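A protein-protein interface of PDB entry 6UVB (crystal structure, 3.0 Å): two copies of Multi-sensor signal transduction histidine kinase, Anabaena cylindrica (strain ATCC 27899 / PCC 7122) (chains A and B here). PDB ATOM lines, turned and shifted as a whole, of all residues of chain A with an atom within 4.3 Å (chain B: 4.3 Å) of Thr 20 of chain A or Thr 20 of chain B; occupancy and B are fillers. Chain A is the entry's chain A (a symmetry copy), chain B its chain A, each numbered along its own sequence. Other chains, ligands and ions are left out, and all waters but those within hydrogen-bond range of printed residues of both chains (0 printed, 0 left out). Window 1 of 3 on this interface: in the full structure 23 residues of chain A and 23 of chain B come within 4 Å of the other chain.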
ATOM      1  N   GLN A  16      19.608   4.219  22.456  1.00  0.00           N
ATOM      2  CA  GLN A  16      19.859   4.380  21.029  1.00  0.00           C
ATOM      3  C   GLN A  16      21.289   4.814  20.756  1.00  0.00           C
ATOM      4  O   GLN A  16      21.867   4.434  19.723  1.00  0.00           O
ATOM      5  CB  GLN A  16      18.888   5.387  20.422  1.00  0.00           C
ATOM      6  CG  GLN A  16      17.456   4.910  20.411  1.00  0.00           C
ATOM      7  CD  GLN A  16      16.638   5.569  21.483  1.00  0.00           C
ATOM      8  OE1 GLN A  16      16.772   6.761  21.715  1.00  0.00           O
ATOM      9  NE2 GLN A  16      15.802   4.795  22.168  1.00  0.00           N
ATOM     10  N   ILE A  17      21.865   5.610  21.663  1.00  0.00           N
ATOM     11  CA  ILE A  17      23.223   6.105  21.470  1.00  0.00           C
ATOM     12  C   ILE A  17      24.231   4.966  21.593  1.00  0.00           C
ATOM     13  O   ILE A  17      24.992   4.696  20.659  1.00  0.00           O
ATOM     14  CB  ILE A  17      23.511   7.250  22.455  1.00  0.00           C
ATOM     15  CG1 ILE A  17      22.637   8.447  22.099  1.00  0.00           C
ATOM     16  CG2 ILE A  17      24.978   7.634  22.447  1.00  0.00           C
ATOM     17  CD1 ILE A  17      23.107   9.741  22.675  1.00  0.00           C
ATOM     18  N   ARG A  18      24.228   4.260  22.733  1.00  0.00           N
ATOM     19  CA  ARG A  18      25.159   3.147  22.923  1.00  0.00           C
ATOM     20  C   ARG A  18      24.892   2.035  21.919  1.00  0.00           C
ATOM     21  O   ARG A  18      25.820   1.332  21.499  1.00  0.00           O
ATOM     22  CB  ARG A  18      25.064   2.610  24.351  1.00  0.00           C
ATOM     23  CG  ARG A  18      24.970   3.705  25.423  1.00  0.00           C
ATOM     24  CD  ARG A  18      26.234   3.825  26.257  1.00  0.00           C
ATOM     25  NE  ARG A  18      26.268   2.832  27.322  1.00  0.00           N
ATOM     26  CZ  ARG A  18      25.984   3.093  28.594  1.00  0.00           C
ATOM     27  NH1 ARG A  18      26.041   2.120  29.490  1.00  0.00           N
ATOM     28  NH2 ARG A  18      25.653   4.323  28.978  1.00  0.00           N
ATOM     29  N   SER A  19      23.626   1.869  21.511  1.00  0.00           N
ATOM     30  CA  SER A  19      23.259   0.942  20.442  1.00  0.00           C
ATOM     31  C   SER A  19      24.006   1.291  19.166  1.00  0.00           C
ATOM     32  O   SER A  19      24.956   0.598  18.789  1.00  0.00           O
ATOM     33  CB  SER A  19      21.750   0.979  20.165  1.00  0.00           C
ATOM     34  OG  SER A  19      21.230  -0.307  19.866  1.00  0.00           O
ATOM     35  N   THR A  20      23.592   2.386  18.520  1.00  0.00           N
ATOM     36  CA  THR A  20      24.107   2.755  17.206  1.00  0.00           C
ATOM     37  C   THR A  20      25.624   2.943  17.191  1.00  0.00           C
ATOM     38  O   THR A  20      26.245   2.755  16.137  1.00  0.00           O
ATOM     39  CB  THR A  20      23.389   4.033  16.719  1.00  0.00           C
ATOM     40  OG1 THR A  20      23.266   4.989  17.790  1.00  0.00           O
ATOM     41  CG2 THR A  20      21.987   3.699  16.217  1.00  0.00           C
ATOM     42  N   LEU A  21      26.237   3.250  18.344  1.00  0.00           N
ATOM     43  CA  LEU A  21      27.629   3.701  18.402  1.00  0.00           C
ATOM     44  C   LEU A  21      28.642   2.610  18.737  1.00  0.00           C
ATOM     45  O   LEU A  21      29.835   2.777  18.440  1.00  0.00           O
ATOM     46  CB  LEU A  21      27.779   4.836  19.427  1.00  0.00           C
ATOM     47  CG  LEU A  21      29.170   5.481  19.554  1.00  0.00           C
ATOM     48  CD1 LEU A  21      29.666   5.937  18.180  1.00  0.00           C
ATOM     49  CD2 LEU A  21      29.194   6.619  20.573  1.00  0.00           C
ATOM     50  N   ASN A  22      28.218   1.511  19.343  1.00  0.00           N
ATOM     51  CA  ASN A  22      29.114   0.378  19.518  1.00  0.00           C
ATOM     52  C   ASN A  22      29.123  -0.463  18.245  1.00  0.00           C
ATOM     53  O   ASN A  22      28.085  -0.644  17.600  1.00  0.00           O
ATOM     54  CB  ASN A  22      28.689  -0.431  20.745  1.00  0.00           C
ATOM     55  CG  ASN A  22      28.475  -1.895  20.451  1.00  0.00           C
ATOM     56  OD1 ASN A  22      27.468  -2.283  19.855  1.00  0.00           O
ATOM     57  ND2 ASN A  22      29.398  -2.726  20.916  1.00  0.00           N
ATOM     58  N   ILE A  26      26.212  -3.149  15.116  1.00  0.00           N
ATOM     59  CA  ILE A  26      25.999  -2.993  13.685  1.00  0.00           C
ATOM     60  C   ILE A  26      26.641  -4.129  12.888  1.00  0.00           C
ATOM     61  O   ILE A  26      26.212  -4.401  11.759  1.00  0.00           O
ATOM     62  CB  ILE A  26      26.455  -1.606  13.184  1.00  0.00           C
ATOM     63  CG1 ILE A  26      27.958  -1.581  12.924  1.00  0.00           C
ATOM     64  CG2 ILE A  26      25.981  -0.473  14.162  1.00  0.00           C
ATOM     65  CD1 ILE A  26      28.483  -0.213  12.548  1.00  0.00           C
ATOM     66  N   GLN B  16      21.256   2.041   6.136  1.00  0.00           N
ATOM     67  CA  GLN B  16      21.390   1.991   7.586  1.00  0.00           C
ATOM     68  C   GLN B  16      22.788   2.381   8.035  1.00  0.00           C
ATOM     69  O   GLN B  16      22.951   2.977   9.114  1.00  0.00           O
ATOM     70  CB  GLN B  16      21.046   0.602   8.112  1.00  0.00           C
ATOM     71  CG  GLN B  16      19.591   0.238   7.943  1.00  0.00           C
ATOM     72  CD  GLN B  16      19.381  -0.720   6.807  1.00  0.00           C
ATOM     73  OE1 GLN B  16      20.158  -1.648   6.633  1.00  0.00           O
ATOM     74  NE2 GLN B  16      18.346  -0.492   6.006  1.00  0.00           N
ATOM     75  N   ILE B  17      23.800   2.046   7.227  1.00  0.00           N
ATOM     76  CA  ILE B  17      25.179   2.349   7.590  1.00  0.00           C
ATOM     77  C   ILE B  17      25.428   3.855   7.545  1.00  0.00           C
ATOM     78  O   ILE B  17      25.814   4.458   8.551  1.00  0.00           O
ATOM     79  CB  ILE B  17      26.145   1.569   6.682  1.00  0.00           C
ATOM     80  CG1 ILE B  17      26.013   0.080   6.977  1.00  0.00           C
ATOM     81  CG2 ILE B  17      27.578   2.029   6.872  1.00  0.00           C
ATOM     82  CD1 ILE B  17      27.165  -0.742   6.501  1.00  0.00           C
ATOM     83  N   ARG B  18      25.178   4.486   6.390  1.00  0.00           N
ATOM     84  CA  ARG B  18      25.384   5.930   6.271  1.00  0.00           C
ATOM     85  C   ARG B  18      24.450   6.693   7.199  1.00  0.00           C
ATOM     86  O   ARG B  18      24.803   7.769   7.699  1.00  0.00           O
ATOM     87  CB  ARG B  18      25.180   6.381   4.823  1.00  0.00           C
ATOM     88  CG  ARG B  18      25.809   5.441   3.786  1.00  0.00           C
ATOM     89  CD  ARG B  18      27.026   6.044   3.106  1.00  0.00           C
ATOM     90  NE  ARG B  18      26.645   6.936   2.018  1.00  0.00           N
ATOM     91  CZ  ARG B  18      26.693   6.607   0.732  1.00  0.00           C
ATOM     92  NH1 ARG B  18      26.322   7.488  -0.184  1.00  0.00           N
ATOM     93  NH2 ARG B  18      27.118   5.403   0.355  1.00  0.00           N
ATOM     94  N   SER B  19      23.255   6.142   7.455  1.00  0.00           N
ATOM     95  CA  SER B  19      22.330   6.692   8.444  1.00  0.00           C
ATOM     96  C   SER B  19      22.996   6.756   9.807  1.00  0.00           C
ATOM     97  O   SER B  19      23.378   7.837  10.267  1.00  0.00           O
ATOM     98  CB  SER B  19      21.055   5.846   8.547  1.00  0.00           C
ATOM     99  OG  SER B  19      19.898   6.643   8.741  1.00  0.00           O
ATOM    100  N   THR B  20      23.162   5.588  10.438  1.00  0.00           N
ATOM    101  CA  THR B  20      23.641   5.508  11.814  1.00  0.00           C
ATOM    102  C   THR B  20      25.009   6.161  12.008  1.00  0.00           C
ATOM    103  O   THR B  20      25.308   6.617  13.119  1.00  0.00           O
ATOM    104  CB  THR B  20      23.667   4.029  12.257  1.00  0.00           C
ATOM    105  OG1 THR B  20      24.198   3.192  11.212  1.00  0.00           O
ATOM    106  CG2 THR B  20      22.257   3.545  12.585  1.00  0.00           C
ATOM    107  N   LEU B  21      25.818   6.268  10.943  1.00  0.00           N
ATOM    108  CA  LEU B  21      27.231   6.634  11.059  1.00  0.00           C
ATOM    109  C   LEU B  21      27.534   8.108  10.806  1.00  0.00           C
ATOM    110  O   LEU B  21      28.588   8.595  11.243  1.00  0.00           O
ATOM    111  CB  LEU B  21      28.081   5.790  10.097  1.00  0.00           C
ATOM    112  CG  LEU B  21      29.605   5.994  10.150  1.00  0.00           C
ATOM    113  CD1 LEU B  21      30.107   5.828  11.587  1.00  0.00           C
ATOM    114  CD2 LEU B  21      30.350   5.080   9.180  1.00  0.00           C
ATOM    115  N   ASN B  22      26.660   8.829  10.120  1.00  0.00           N
ATOM    116  CA  ASN B  22      26.824  10.270  10.011  1.00  0.00           C
ATOM    117  C   ASN B  22      26.237  10.943  11.248  1.00  0.00           C
ATOM    118  O   ASN B  22      25.197  10.519  11.763  1.00  0.00           O
ATOM    119  CB  ASN B  22      26.175  10.767   8.717  1.00  0.00           C
ATOM    120  CG  ASN B  22      25.180  11.879   8.936  1.00  0.00           C
ATOM    121  OD1 ASN B  22      24.061  11.648   9.399  1.00  0.00           O
ATOM    122  ND2 ASN B  22      25.561  13.090   8.552  1.00  0.00           N
ATOM    123  N   ILE B  26      22.006  11.550  13.932  1.00  0.00           N
ATOM    124  CA  ILE B  26      21.747  11.257  15.335  1.00  0.00           C
ATOM    125  C   ILE B  26      21.586  12.532  16.162  1.00  0.00           C
ATOM    126  O   ILE B  26      20.952  12.495  17.224  1.00  0.00           O
ATOM    127  CB  ILE B  26      22.814  10.313  15.929  1.00  0.00           C
ATOM    128  CG1 ILE B  26      24.056  11.087  16.361  1.00  0.00           C
ATOM    129  CG2 ILE B  26      23.134   9.135  14.942  1.00  0.00           C
ATOM    130  CD1 ILE B  26      25.184  10.200  16.840  1.00  0.00           C
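Thr 20 of chain A touches its own counterpart, Thr 20 of chain B. Positions printed for both chains: 16, 17, 18, 19, 20, 21, 22 and 26.
Printed residues of chain B that touch a printed residue of chain A: Thr 20.
CG2 of Thr 20 of chain B touches CG2 of Thr 20 of chain A, 3.6 Å away.
O of Gln 16 of chain B lies within hydrogen-bond range of OG1 of Thr 20 of chain B (2.5 Å). O of Ile 17 of chain A sits at hydrogen-bond distance from OG1 of Thr 20 of chain A, 3.4 Å away. O of Ile 17 of chain B is in hydrogen-bond range of OG1 of Thr 20 of chain B, at 3.4 Å. O of Gln 16 of chain A is in hydrogen-bond range of OG1 of Thr 20 of chain A, 2.4 Å away.
Of chain B, only Thr 20 comes within 4 Å of Thr 20 of chain A. Thr 20 of chain B touches just one residue of chain A: Thr 20 (3.6 Å). Ile 17 of chain B touches none of the printed residues of chain A. The nearest printed residue of chain B that does not touch Thr 20 of chain A is Ile 26 of chain B (5.0 Å). The nearest printed residue of chain A that does not touch Thr 20 of chain B is Ile 26 of chain A (5.0 Å).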
